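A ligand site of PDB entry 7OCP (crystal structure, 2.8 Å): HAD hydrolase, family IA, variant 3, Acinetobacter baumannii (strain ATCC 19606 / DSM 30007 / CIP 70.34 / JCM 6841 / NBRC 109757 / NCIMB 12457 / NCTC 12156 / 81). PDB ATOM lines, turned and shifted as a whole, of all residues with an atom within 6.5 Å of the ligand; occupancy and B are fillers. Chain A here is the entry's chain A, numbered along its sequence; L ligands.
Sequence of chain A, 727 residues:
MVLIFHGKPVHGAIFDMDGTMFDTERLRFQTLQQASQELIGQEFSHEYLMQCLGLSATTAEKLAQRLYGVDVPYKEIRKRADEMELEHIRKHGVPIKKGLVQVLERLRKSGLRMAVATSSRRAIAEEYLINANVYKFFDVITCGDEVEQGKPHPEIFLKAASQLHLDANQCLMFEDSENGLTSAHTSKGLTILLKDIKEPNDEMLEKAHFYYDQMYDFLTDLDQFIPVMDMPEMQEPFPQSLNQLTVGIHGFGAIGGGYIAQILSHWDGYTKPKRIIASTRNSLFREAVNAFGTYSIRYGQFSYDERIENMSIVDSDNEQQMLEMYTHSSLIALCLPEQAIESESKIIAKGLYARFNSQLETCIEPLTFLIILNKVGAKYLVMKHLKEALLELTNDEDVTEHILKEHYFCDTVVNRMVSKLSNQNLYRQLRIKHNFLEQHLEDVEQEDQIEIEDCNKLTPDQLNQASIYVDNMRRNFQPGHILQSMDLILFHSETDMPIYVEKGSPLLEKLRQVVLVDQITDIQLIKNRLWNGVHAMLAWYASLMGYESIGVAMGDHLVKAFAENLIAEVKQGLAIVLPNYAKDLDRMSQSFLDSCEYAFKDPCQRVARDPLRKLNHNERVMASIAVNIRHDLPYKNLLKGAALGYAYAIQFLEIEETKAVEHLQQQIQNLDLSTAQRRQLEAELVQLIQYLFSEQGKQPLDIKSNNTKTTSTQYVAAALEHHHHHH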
ATOM      1  N   HIS A 250     -22.225  -3.366   9.084  1.00  0.00           N
ATOM      2  CA  HIS A 250     -21.271  -3.591   7.970  1.00  0.00           C
ATOM      3  C   HIS A 250     -20.225  -4.627   8.418  1.00  0.00           C
ATOM      4  O   HIS A 250     -19.228  -4.226   9.045  1.00  0.00           O
ATOM      5  CB  HIS A 250     -20.633  -2.269   7.513  1.00  0.00           C
ATOM      6  CG  HIS A 250     -19.925  -2.349   6.207  1.00  0.00           C
ATOM      7  ND1 HIS A 250     -20.240  -1.542   5.148  1.00  0.00           N
ATOM      8  CD2 HIS A 250     -18.921  -3.152   5.788  1.00  0.00           C
ATOM      9  CE1 HIS A 250     -19.458  -1.830   4.121  1.00  0.00           C
ATOM     10  NE2 HIS A 250     -18.637  -2.819   4.494  1.00  0.00           N
ATOM     11  N   GLY A 251     -20.486  -5.904   8.125  1.00  0.00           N
ATOM     12  CA  GLY A 251     -19.644  -7.044   8.533  1.00  0.00           C
ATOM     13  C   GLY A 251     -20.344  -7.875   9.606  1.00  0.00           C
ATOM     14  O   GLY A 251     -19.998  -7.714  10.796  1.00  0.00           O
ATOM     15  N   PHE A 252     -21.284  -8.724   9.191  1.00  0.00           N
ATOM     16  CA  PHE A 252     -22.011  -9.693  10.044  1.00  0.00           C
ATOM     17  C   PHE A 252     -21.036 -10.789  10.492  1.00  0.00           C
ATOM     18  O   PHE A 252     -21.166 -11.939  10.041  1.00  0.00           O
ATOM     19  CB  PHE A 252     -23.224 -10.259   9.298  1.00  0.00           C
ATOM     20  CG  PHE A 252     -24.157 -11.115  10.119  1.00  0.00           C
ATOM     21  CD1 PHE A 252     -24.807 -10.586  11.218  1.00  0.00           C
ATOM     22  CD2 PHE A 252     -24.384 -12.442   9.790  1.00  0.00           C
ATOM     23  CE1 PHE A 252     -25.671 -11.369  11.979  1.00  0.00           C
ATOM     24  CE2 PHE A 252     -25.245 -13.218  10.544  1.00  0.00           C
ATOM     25  CZ  PHE A 252     -25.880 -12.688  11.636  1.00  0.00           C
ATOM     26  N   GLY A 253     -20.077 -10.409  11.346  1.00  0.00           N
ATOM     27  CA  GLY A 253     -19.057 -11.306  11.906  1.00  0.00           C
ATOM     28  C   GLY A 253     -19.306 -11.576  13.377  1.00  0.00           C
ATOM     29  O   GLY A 253     -20.436 -11.311  13.832  1.00  0.00           O
ATOM     30  N   ALA A 254     -18.292 -12.069  14.084  1.00  0.00           N
ATOM     31  CA  ALA A 254     -18.346 -12.403  15.529  1.00  0.00           C
ATOM     32  C   ALA A 254     -18.904 -11.197  16.308  1.00  0.00           C
ATOM     33  O   ALA A 254     -19.990 -11.339  16.906  1.00  0.00           O
ATOM     34  CB  ALA A 254     -16.976 -12.795  16.028  1.00  0.00           C
ATOM     35  N   ILE A 255     -18.214 -10.063  16.258  1.00  0.00           N
ATOM     36  CA  ILE A 255     -18.526  -8.855  17.082  1.00  0.00           C
ATOM     37  C   ILE A 255     -19.769  -8.159  16.525  1.00  0.00           C
ATOM     38  O   ILE A 255     -20.518  -7.572  17.319  1.00  0.00           O
ATOM     39  CB  ILE A 255     -17.300  -7.907  17.171  1.00  0.00           C
ATOM     40  CG1 ILE A 255     -17.278  -7.147  18.495  1.00  0.00           C
ATOM     41  CG2 ILE A 255     -17.228  -6.981  15.964  1.00  0.00           C
ATOM     42  CD1 ILE A 255     -16.979  -8.011  19.697  1.00  0.00           C
ATOM     43  N   GLY A 256     -19.980  -8.219  15.198  1.00  0.00           N
ATOM     44  CA  GLY A 256     -21.141  -7.620  14.521  1.00  0.00           C
ATOM     45  C   GLY A 256     -22.443  -8.313  14.898  1.00  0.00           C
ATOM     46  O   GLY A 256     -23.371  -7.619  15.345  1.00  0.00           O
ATOM     47  N   SER A 279     -24.165  -7.264   6.523  1.00  0.00           N
ATOM     48  CA  SER A 279     -23.454  -7.667   5.281  1.00  0.00           C
ATOM     49  C   SER A 279     -22.468  -8.809   5.572  1.00  0.00           C
ATOM     50  O   SER A 279     -21.712  -8.691   6.552  1.00  0.00           O
ATOM     51  CB  SER A 279     -22.749  -6.478   4.663  1.00  0.00           C
ATOM     52  OG  SER A 279     -21.689  -6.038   5.486  1.00  0.00           O
ATOM     53  N   THR A 280     -22.483  -9.846   4.738  1.00  0.00           N
ATOM     54  CA  THR A 280     -21.527 -10.986   4.785  1.00  0.00           C
ATOM     55  C   THR A 280     -21.363 -11.574   3.371  1.00  0.00           C
ATOM     56  O   THR A 280     -22.352 -11.553   2.607  1.00  0.00           O
ATOM     57  CB  THR A 280     -21.981 -12.052   5.787  1.00  0.00           C
ATOM     58  OG1 THR A 280     -21.014 -13.110   5.788  1.00  0.00           O
ATOM     59  CG2 THR A 280     -23.350 -12.629   5.477  1.00  0.00           C
ATOM     60  N   ARG A 281     -20.166 -12.066   3.058  1.00  0.00           N
ATOM     61  CA  ARG A 281     -19.842 -12.787   1.798  1.00  0.00           C
ATOM     62  C   ARG A 281     -20.252 -14.259   1.952  1.00  0.00           C
ATOM     63  O   ARG A 281     -20.451 -14.929   0.907  1.00  0.00           O
ATOM     64  CB  ARG A 281     -18.355 -12.660   1.466  1.00  0.00           C
ATOM     65  CG  ARG A 281     -17.817 -11.232   1.467  1.00  0.00           C
ATOM     66  CD  ARG A 281     -16.297 -11.191   1.517  1.00  0.00           C
ATOM     67  NE  ARG A 281     -15.759 -11.724   2.763  1.00  0.00           N
ATOM     68  CZ  ARG A 281     -14.483 -12.009   2.991  1.00  0.00           C
ATOM     69  NH1 ARG A 281     -14.121 -12.486   4.175  1.00  0.00           N
ATOM     70  NH2 ARG A 281     -13.573 -11.809   2.057  1.00  0.00           N
ATOM     71  N   ASN A 282     -20.378 -14.728   3.191  1.00  0.00           N
ATOM     72  CA  ASN A 282     -20.783 -16.116   3.561  1.00  0.00           C
ATOM     73  C   ASN A 282     -22.249 -16.336   3.153  1.00  0.00           C
ATOM     74  O   ASN A 282     -23.140 -15.795   3.844  1.00  0.00           O
ATOM     75  CB  ASN A 282     -20.566 -16.372   5.063  1.00  0.00           C
ATOM     76  CG  ASN A 282     -20.698 -17.821   5.455  1.00  0.00           C
ATOM     77  OD1 ASN A 282     -21.554 -18.543   4.937  1.00  0.00           O
ATOM     78  ND2 ASN A 282     -19.871 -18.267   6.393  1.00  0.00           N
ATOM     79  N   SER A 316     -22.314  -8.678   0.626  1.00  0.00           N
ATOM     80  CA  SER A 316     -21.357  -7.549   0.666  1.00  0.00           C
ATOM     81  C   SER A 316     -21.023  -7.075  -0.760  1.00  0.00           C
ATOM     82  O   SER A 316     -20.779  -5.872  -0.940  1.00  0.00           O
ATOM     83  CB  SER A 316     -20.112  -7.910   1.436  1.00  0.00           C
ATOM     84  OG  SER A 316     -20.420  -8.247   2.773  1.00  0.00           O
ATOM     85  N   LEU A 334     -19.421  -0.421  11.662  1.00  0.00           N
ATOM     86  CA  LEU A 334     -18.352  -1.069  10.852  1.00  0.00           C
ATOM     87  C   LEU A 334     -17.619  -2.085  11.747  1.00  0.00           C
ATOM     88  O   LEU A 334     -16.903  -1.642  12.664  1.00  0.00           O
ATOM     89  CB  LEU A 334     -17.396   0.006  10.328  1.00  0.00           C
ATOM     90  CG  LEU A 334     -16.418  -0.455   9.255  1.00  0.00           C
ATOM     91  CD1 LEU A 334     -17.133  -0.709   7.939  1.00  0.00           C
ATOM     92  CD2 LEU A 334     -15.298   0.553   9.068  1.00  0.00           C
ATOM     93  N   CYS A 335     -17.801  -3.376  11.486  1.00  0.00           N
ATOM     94  CA  CYS A 335     -17.271  -4.510  12.284  1.00  0.00           C
ATOM     95  C   CYS A 335     -16.325  -5.358  11.431  1.00  0.00           C
ATOM     96  O   CYS A 335     -16.506  -6.594  11.385  1.00  0.00           O
ATOM     97  CB  CYS A 335     -18.414  -5.354  12.841  1.00  0.00           C
ATOM     98  SG  CYS A 335     -19.629  -4.379  13.781  1.00  0.00           S
ATOM     99  N   LEU A 336     -15.332  -4.708  10.797  1.00  0.00           N
ATOM    100  CA  LEU A 336     -14.337  -5.349   9.891  1.00  0.00           C
ATOM    101  C   LEU A 336     -12.985  -5.438  10.591  1.00  0.00           C
ATOM    102  O   LEU A 336     -12.705  -4.646  11.482  1.00  0.00           O
ATOM    103  CB  LEU A 336     -14.233  -4.528   8.608  1.00  0.00           C
ATOM    104  CG  LEU A 336     -15.531  -4.311   7.836  1.00  0.00           C
ATOM    105  CD1 LEU A 336     -15.301  -3.375   6.659  1.00  0.00           C
ATOM    106  CD2 LEU A 336     -16.104  -5.638   7.351  1.00  0.00           C
ATOM    107  N   PRO A 337     -12.113  -6.390  10.204  1.00  0.00           N
ATOM    108  CA  PRO A 337     -10.700  -6.370  10.613  1.00  0.00           C
ATOM    109  C   PRO A 337      -9.946  -5.210   9.943  1.00  0.00           C
ATOM    110  O   PRO A 337     -10.498  -4.602   9.044  1.00  0.00           O
ATOM    111  CB  PRO A 337     -10.132  -7.718  10.136  1.00  0.00           C
ATOM    112  CG  PRO A 337     -11.344  -8.559   9.793  1.00  0.00           C
ATOM    113  CD  PRO A 337     -12.421  -7.578   9.395  1.00  0.00           C
ATOM    114  N   GLU A 338      -8.700  -4.966  10.373  1.00  0.00           N
ATOM    115  CA  GLU A 338      -7.843  -3.852   9.861  1.00  0.00           C
ATOM    116  C   GLU A 338      -7.559  -4.046   8.372  1.00  0.00           C
ATOM    117  O   GLU A 338      -7.610  -3.050   7.634  1.00  0.00           O
ATOM    118  CB  GLU A 338      -6.537  -3.778  10.659  1.00  0.00           C
ATOM    119  CG  GLU A 338      -5.771  -2.481  10.449  1.00  0.00           C
ATOM    120  CD  GLU A 338      -4.311  -2.513  10.856  1.00  0.00           C
ATOM    121  OE1 GLU A 338      -3.960  -3.306  11.755  1.00  0.00           O
ATOM    122  OE2 GLU A 338      -3.516  -1.747  10.270  1.00  0.00           O
ATOM    123  N   GLN A 339      -7.262  -5.293   7.956  1.00  0.00           N
ATOM    124  CA  GLN A 339      -6.841  -5.636   6.566  1.00  0.00           C
ATOM    125  C   GLN A 339      -7.978  -5.381   5.576  1.00  0.00           C
ATOM    126  O   GLN A 339      -7.676  -5.096   4.403  1.00  0.00           O
ATOM    127  CB  GLN A 339      -6.347  -7.090   6.481  1.00  0.00           C
ATOM    128  CG  GLN A 339      -7.376  -8.137   6.900  1.00  0.00           C
ATOM    129  CD  GLN A 339      -7.145  -8.670   8.297  1.00  0.00           C
ATOM    130  OE1 GLN A 339      -6.871  -7.910   9.227  1.00  0.00           O
ATOM    131  NE2 GLN A 339      -7.283  -9.969   8.454  1.00  0.00           N
ATOM    132  N   ALA A 340      -9.241  -5.486   6.021  1.00  0.00           N
ATOM    133  CA  ALA A 340     -10.459  -5.352   5.186  1.00  0.00           C
ATOM    134  C   ALA A 340     -10.805  -3.873   4.962  1.00  0.00           C
ATOM    135  O   ALA A 340     -11.551  -3.601   3.990  1.00  0.00           O
ATOM    136  CB  ALA A 340     -11.596  -6.091   5.834  1.00  0.00           C
ATOM    137  N   SER A 343      -9.964  -2.365   1.270  1.00  0.00           N
ATOM    138  CA  SER A 343     -10.816  -2.911   0.181  1.00  0.00           C
ATOM    139  C   SER A 343     -12.263  -2.414   0.338  1.00  0.00           C
ATOM    140  O   SER A 343     -12.872  -2.052  -0.695  1.00  0.00           O
ATOM    141  CB  SER A 343     -10.750  -4.417   0.132  1.00  0.00           C
ATOM    142  OG  SER A 343     -11.334  -4.991   1.300  1.00  0.00           O
ATOM    143  N   GLU A 344     -12.780  -2.391   1.564  1.00  0.00           N
ATOM    144  CA  GLU A 344     -14.203  -2.073   1.877  1.00  0.00           C
ATOM    145  C   GLU A 344     -14.420  -0.561   1.957  1.00  0.00           C
ATOM    146  O   GLU A 344     -15.587  -0.145   2.091  1.00  0.00           O
ATOM    147  CB  GLU A 344     -14.633  -2.754   3.178  1.00  0.00           C
ATOM    148  CG  GLU A 344     -14.744  -4.262   3.069  1.00  0.00           C
ATOM    149  CD  GLU A 344     -15.936  -4.760   2.267  1.00  0.00           C
ATOM    150  OE1 GLU A 344     -15.719  -5.536   1.317  1.00  0.00           O
ATOM    151  OE2 GLU A 344     -17.075  -4.388   2.603  1.00  0.00           O
ATOM    152  N   ILE A 372     -15.910  -0.200  15.070  1.00  0.00           N
ATOM    153  CA  ILE A 372     -15.629  -1.397  15.908  1.00  0.00           C
ATOM    154  C   ILE A 372     -14.307  -2.009  15.412  1.00  0.00           C
ATOM    155  O   ILE A 372     -14.334  -2.746  14.400  1.00  0.00           O
ATOM    156  CB  ILE A 372     -16.790  -2.409  15.870  1.00  0.00           C
ATOM    157  CG1 ILE A 372     -18.160  -1.729  16.034  1.00  0.00           C
ATOM    158  CG2 ILE A 372     -16.584  -3.515  16.898  1.00  0.00           C
ATOM    159  CD1 ILE A 372     -18.283  -0.877  17.272  1.00  0.00           C
ATOM    160  N   LEU A 373     -13.200  -1.696  16.085  1.00  0.00           N
ATOM    161  CA  LEU A 373     -11.834  -2.129  15.709  1.00  0.00           C
ATOM    162  C   LEU A 373     -10.894  -1.960  16.918  1.00  0.00           C
ATOM    163  O   LEU A 373     -10.664  -0.810  17.322  1.00  0.00           O
ATOM    164  CB  LEU A 373     -11.359  -1.286  14.513  1.00  0.00           C
ATOM    165  CG  LEU A 373      -9.898  -1.438  14.101  1.00  0.00           C
ATOM    166  CD1 LEU A 373      -9.508  -2.903  13.918  1.00  0.00           C
ATOM    167  CD2 LEU A 373      -9.613  -0.664  12.832  1.00  0.00           C
ATOM    168  N   ASN A 374     -10.399  -3.086  17.461  1.00  0.00           N
ATOM    169  CA  ASN A 374      -9.512  -3.134  18.653  1.00  0.00           C
ATOM    170  C   ASN A 374      -8.105  -2.685  18.225  1.00  0.00           C
ATOM    171  O   ASN A 374      -7.231  -3.561  18.045  1.00  0.00           O
ATOM    172  CB  ASN A 374      -9.526  -4.522  19.299  1.00  0.00           C
ATOM    173  CG  ASN A 374      -8.785  -4.588  20.619  1.00  0.00           C
ATOM    174  OD1 ASN A 374      -8.416  -3.565  21.190  1.00  0.00           O
ATOM    175  ND2 ASN A 374      -8.584  -5.793  21.124  1.00  0.00           N
ATOM    176  N   LYS A 375      -7.914  -1.370  18.075  1.00  0.00           N
ATOM    177  CA  LYS A 375      -6.640  -0.763  17.617  1.00  0.00           C
ATOM    178  C   LYS A 375      -6.640   0.736  17.948  1.00  0.00           C
ATOM    179  O   LYS A 375      -7.724   1.351  17.918  1.00  0.00           O
ATOM    180  CB  LYS A 375      -6.461  -0.986  16.114  1.00  0.00           C
ATOM    181  CG  LYS A 375      -5.024  -1.052  15.617  1.00  0.00           C
ATOM    182  CD  LYS A 375      -4.801  -2.068  14.522  1.00  0.00           C
ATOM    183  CE  LYS A 375      -4.775  -3.489  15.036  1.00  0.00           C
ATOM    184  NZ  LYS A 375      -4.994  -4.482  13.958  1.00  0.00           N
ATOM    185  N   VAL A 414     -14.475  -1.948  22.730  1.00  0.00           N
ATOM    186  CA  VAL A 414     -15.300  -3.164  22.950  1.00  0.00           C
ATOM    187  C   VAL A 414     -14.486  -4.154  23.802  1.00  0.00           C
ATOM    188  O   VAL A 414     -13.276  -4.301  23.526  1.00  0.00           O
ATOM    189  CB  VAL A 414     -15.750  -3.794  21.622  1.00  0.00           C
ATOM    190  CG1 VAL A 414     -16.390  -5.154  21.821  1.00  0.00           C
ATOM    191  CG2 VAL A 414     -16.676  -2.853  20.853  1.00  0.00           C
ATOM    192  N   ASN A 415     -15.131  -4.779  24.792  1.00  0.00           N
ATOM    193  CA  ASN A 415     -14.478  -5.696  25.766  1.00  0.00           C
ATOM    194  C   ASN A 415     -14.991  -7.135  25.589  1.00  0.00           C
ATOM    195  O   ASN A 415     -14.235  -8.060  25.969  1.00  0.00           O
ATOM    196  CB  ASN A 415     -14.678  -5.209  27.213  1.00  0.00           C
ATOM    197  CG  ASN A 415     -13.830  -3.994  27.540  1.00  0.00           C
ATOM    198  OD1 ASN A 415     -12.677  -3.912  27.144  1.00  0.00           O
ATOM    199  ND2 ASN A 415     -14.403  -3.060  28.279  1.00  0.00           N
ATOM    200  N   ARG A 416     -16.188  -7.337  25.046  1.00  0.00           N
ATOM    201  CA  ARG A 416     -16.806  -8.681  24.875  1.00  0.00           C
ATOM    202  C   ARG A 416     -16.010  -9.485  23.844  1.00  0.00           C
ATOM    203  O   ARG A 416     -15.950  -9.043  22.682  1.00  0.00           O
ATOM    204  CB  ARG A 416     -18.272  -8.573  24.453  1.00  0.00           C
ATOM    205  CG  ARG A 416     -18.965  -9.931  24.311  1.00  0.00           C
ATOM    206  CD  ARG A 416     -20.424  -9.824  23.935  1.00  0.00           C
ATOM    207  NE  ARG A 416     -21.252  -9.299  25.016  1.00  0.00           N
ATOM    208  CZ  ARG A 416     -22.574  -9.252  25.002  1.00  0.00           C
ATOM    209  NH1 ARG A 416     -23.262  -9.698  23.961  1.00  0.00           N
ATOM    210  NH2 ARG A 416     -23.224  -8.757  26.053  1.00  0.00           N
ATOM    211  N   MET A 417     -15.445 -10.625  24.256  1.00  0.00           N
ATOM    212  CA  MET A 417     -14.856 -11.647  23.364  1.00  0.00           C
ATOM    213  C   MET A 417     -15.991 -12.485  22.777  1.00  0.00           C
ATOM    214  O   MET A 417     -16.828 -12.966  23.568  1.00  0.00           O
ATOM    215  CB  MET A 417     -13.892 -12.570  24.123  1.00  0.00           C
ATOM    216  CG  MET A 417     -12.616 -11.889  24.570  1.00  0.00           C
ATOM    217  SD  MET A 417     -11.491 -13.048  25.397  1.00  0.00           S
ATOM    218  CE  MET A 417     -10.016 -12.037  25.564  1.00  0.00           C
ATOM    219  N   VAL A 418     -16.024 -12.651  21.448  1.00  0.00           N
ATOM    220  CA  VAL A 418     -17.073 -13.430  20.721  1.00  0.00           C
ATOM    221  C   VAL A 418     -16.388 -14.424  19.778  1.00  0.00           C
ATOM    222  O   VAL A 418     -15.316 -14.097  19.239  1.00  0.00           O
ATOM    223  CB  VAL A 418     -18.029 -12.507  19.950  1.00  0.00           C
ATOM    224  CG1 VAL A 418     -19.166 -13.295  19.310  1.00  0.00           C
ATOM    225  CG2 VAL A 418     -18.570 -11.387  20.827  1.00  0.00           C
ATOM    226  N   SER A 419     -17.008 -15.592  19.590  1.00  0.00           N
ATOM    227  CA  SER A 419     -16.578 -16.681  18.669  1.00  0.00           C
ATOM    228  C   SER A 419     -17.676 -16.937  17.632  1.00  0.00           C
ATOM    229  O   SER A 419     -18.831 -17.169  18.041  1.00  0.00           O
ATOM    230  CB  SER A 419     -16.245 -17.937  19.441  1.00  0.00           C
ATOM    231  OG  SER A 419     -15.829 -18.973  18.566  1.00  0.00           O
ATOM    232  N   LYS A 420     -17.326 -16.883  16.340  1.00  0.00           N
ATOM    233  CA  LYS A 420     -18.240 -17.155  15.202  1.00  0.00           C
ATOM    234  C   LYS A 420     -18.220 -18.660  14.916  1.00  0.00           C
ATOM    235  O   LYS A 420     -17.111 -19.233  14.852  1.00  0.00           O
ATOM    236  CB  LYS A 420     -17.813 -16.336  13.977  1.00  0.00           C
ATOM    237  CG  LYS A 420     -18.661 -16.541  12.727  1.00  0.00           C
ATOM    238  CD  LYS A 420     -18.338 -15.547  11.631  1.00  0.00           C
ATOM    239  CE  LYS A 420     -18.888 -15.957  10.274  1.00  0.00           C
ATOM    240  NZ  LYS A 420     -18.712 -14.877   9.274  1.00  0.00           N
ATOM    241  N   LYS A 527      -7.969  -0.208  28.183  1.00  0.00           N
ATOM    242  CA  LYS A 527      -8.105  -1.333  27.228  1.00  0.00           C
ATOM    243  C   LYS A 527      -6.716  -1.839  26.819  1.00  0.00           C
ATOM    244  O   LYS A 527      -6.533  -3.066  26.699  1.00  0.00           O
ATOM    245  CB  LYS A 527      -8.914  -0.898  26.010  1.00  0.00           C
ATOM    246  CG  LYS A 527      -9.087  -1.944  24.913  1.00  0.00           C
ATOM    247  CD  LYS A 527      -9.765  -3.196  25.392  1.00  0.00           C
ATOM    248  CE  LYS A 527     -10.169  -4.119  24.262  1.00  0.00           C
ATOM    249  NZ  LYS A 527     -10.990  -5.254  24.739  1.00  0.00           N
HETATM  250  P1  LIG L   1     -14.291 -11.641  11.561  1.00  0.00           P
HETATM  251  O1  LIG L   1     -12.995 -12.316  11.284  1.00  0.00           O
HETATM  252  O2  LIG L   1     -15.382 -12.362  12.303  1.00  0.00           O
HETATM  253  O3  LIG L   1     -14.875 -11.036  10.134  1.00  0.00           O
HETATM  254  C1  LIG L   1     -15.599  -9.875  10.480  1.00  0.00           C
HETATM  255  C2  LIG L   1     -16.284  -9.310   9.250  1.00  0.00           C
HETATM  256  O4  LIG L   1     -15.307  -8.769   8.385  1.00  0.00           O
HETATM  257  C3  LIG L   1     -17.072 -10.435   8.523  1.00  0.00           C
HETATM  258  O5  LIG L   1     -18.332  -9.964   8.148  1.00  0.00           O
HETATM  259  C4  LIG L   1     -16.216 -10.693   7.250  1.00  0.00           C
HETATM  260  O6  LIG L   1     -16.936 -10.942   6.156  1.00  0.00           O
HETATM  261  C5  LIG L   1     -15.503  -9.303   7.095  1.00  0.00           C
HETATM  262  N1  LIG L   1     -14.160  -9.445   6.485  1.00  0.00           N
HETATM  263  C6  LIG L   1     -13.013 -10.022   7.060  1.00  0.00           C
HETATM  264  N2  LIG L   1     -11.937  -9.994   6.245  1.00  0.00           N
HETATM  265  C7  LIG L   1     -12.414  -9.372   5.084  1.00  0.00           C
HETATM  266  C8  LIG L   1     -11.778  -9.040   3.874  1.00  0.00           C
HETATM  267  N3  LIG L   1     -10.452  -9.349   3.677  1.00  0.00           N
HETATM  268  N4  LIG L   1     -12.462  -8.399   2.851  1.00  0.00           N
HETATM  269  C9  LIG L   1     -13.788  -8.124   3.117  1.00  0.00           C
HETATM  270  N5  LIG L   1     -14.533  -8.368   4.221  1.00  0.00           N
HETATM  271  C10 LIG L   1     -13.805  -9.014   5.214  1.00  0.00           C
HETATM  272  O7  LIG L   1     -13.741 -10.371  12.492  1.00  0.00           O
HETATM  273  P2  LIG L   1     -14.481 -10.332  13.904  1.00  0.00           P
HETATM  274  O8  LIG L   1     -15.906  -9.981  13.723  1.00  0.00           O
HETATM  275  O9  LIG L   1     -14.006 -11.396  14.866  1.00  0.00           O
HETATM  276  O10 LIG L   1     -13.908  -8.878  14.734  1.00  0.00           O
HETATM  277  C11 LIG L   1     -14.114  -7.793  13.889  1.00  0.00           C
HETATM  278  C12 LIG L   1     -13.541  -6.559  14.561  1.00  0.00           C
HETATM  279  O11 LIG L   1     -13.874  -6.592  15.954  1.00  0.00           O
HETATM  280  C13 LIG L   1     -11.980  -6.604  14.457  1.00  0.00           C
HETATM  281  O12 LIG L   1     -11.557  -5.373  13.954  1.00  0.00           O
HETATM  282  C14 LIG L   1     -11.524  -6.820  15.905  1.00  0.00           C
HETATM  283  O13 LIG L   1     -10.389  -6.090  16.255  1.00  0.00           O
HETATM  284  C15 LIG L   1     -12.735  -6.237  16.696  1.00  0.00           C
HETATM  285  N6  LIG L   1     -12.847  -6.857  18.042  1.00  0.00           N
HETATM  286  C16 LIG L   1     -12.987  -8.232  18.168  1.00  0.00           C
HETATM  287  C17 LIG L   1     -13.329  -8.779  19.359  1.00  0.00           C
HETATM  288  C18 LIG L   1     -13.602 -10.214  19.373  1.00  0.00           C
HETATM  289  O14 LIG L   1     -13.095 -11.019  20.177  1.00  0.00           O
HETATM  290  N7  LIG L   1     -14.479 -10.710  18.424  1.00  0.00           N
HETATM  291  C19 LIG L   1     -13.215  -8.018  20.648  1.00  0.00           C
HETATM  292  C20 LIG L   1     -12.798  -6.604  20.426  1.00  0.00           C
HETATM  293  C21 LIG L   1     -12.835  -6.046  19.207  1.00  0.00           C
HETATM  294  P3  LIG L   1     -17.634 -12.643   6.099  1.00  0.00           P
HETATM  295  O15 LIG L   1     -18.746 -12.427   7.066  1.00  0.00           O
HETATM  296  O16 LIG L   1     -18.018 -12.801   4.619  1.00  0.00           O
HETATM  297  O17 LIG L   1     -16.438 -13.411   6.580  1.00  0.00           O
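OG1 of Thr 280 is in hydrogen-bond range of N of Asn 282, at 3.1 Å. OG of Ser 316 lies within hydrogen-bond range of N of Thr 280. N of Gly 251 sits at hydrogen-bond distance from OG of Ser 279, 2.9 Å away. The backbone carbonyl oxygen (O) of Ser 279 lies within hydrogen-bond range of the backbone NH (N) of Phe 252. The backbone NH of Cys 335 is in hydrogen-bond range of the backbone carbonyl oxygen of His 250 (3.0 Å). The backbone carbonyl oxygen (O) of Ala 340 sits at hydrogen-bond distance from the side-chain hydroxyl (OG) of Ser 343. The backbone carbonyl oxygen (O) of Leu 334 sits at hydrogen-bond distance from the backbone NH (N) of Ile 372. O of Val 414 lies within hydrogen-bond range of NZ of Lys 527 (2.8 Å).
Gly 251 touches the ligand (CA to O5, 3.2 Å). Gly 253 touches the ligand. O of Ser 279 touches O5 of the ligand, at 3.9 Å. Cys 335 touches the ligand (O to C2, 3.5 Å). Pro 337 touches the ligand. CB of Ala 340 touches C7 of the ligand, 3.5 Å away. Ser 343 touches the ligand. OE1 of Glu 344 touches C9 of the ligand (3.7 Å). Ile 372 touches the ligand. Leu 373 touches the ligand (CD1 to O12, 3.2 Å). Val 414 touches the ligand (O to C20, 3.9 Å). Arg 416 touches the ligand (O to C19, 3.6 Å). Met 417 touches the ligand (CA to O14, 3.7 Å). Val 418 touches the ligand (O to N7, 3.6 Å). Hydrophobic or aromatic side chains within 4 Å of the ligand: Ala 254, Ile 255, Leu 336, Pro 337, Ala 340 and Leu 373. 23 residues have an atom within 4 Å of the ligand: Gly 251, Phe 252, Gly 253, Ala 254, Ile 255, Ser 279, Thr 280, Arg 281, Asn 282, Cys 335, Leu 336, Pro 337, Ala 340, Ser 343, Glu 344, Ile 372, Leu 373, Asn 374, Val 414, Arg 416, Met 417, Val 418 and Lys 420. The nearest printed residue that does not touch the ligand is Glu 338 (4.6 Å).
The side-chain hydroxyl (OG1) of Thr 280 sits at hydrogen-bond distance from an oxygen (O15) of the ligand (2.7 Å). O16 of the ligand is in hydrogen-bond range of N of Arg 281, 2.8 Å away. An oxygen (O16) of the ligand is in salt-bridge range of the guanidinium group (NE) of Arg 281 (3.1 Å). The backbone carbonyl oxygen of Leu 336 sits at hydrogen-bond distance from an oxygen (O12) of the ligand. The backbone NH (N) of Ala 254 sits at hydrogen-bond distance from an oxygen (O8) of the ligand (3.2 Å). N of Asn 374 sits at hydrogen-bond distance from O13 of the ligand (3.2 Å). O15 of the ligand lies within salt-bridge range of NZ of Lys 420. N of Asn 282 lies within hydrogen-bond range of O16 of the ligand (3.4 Å). The backbone NH (N) of Phe 252 is in hydrogen-bond range of an oxygen (O5) of the ligand. O8 of the ligand sits at hydrogen-bond distance from N of Ile 255, 3.4 Å away.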
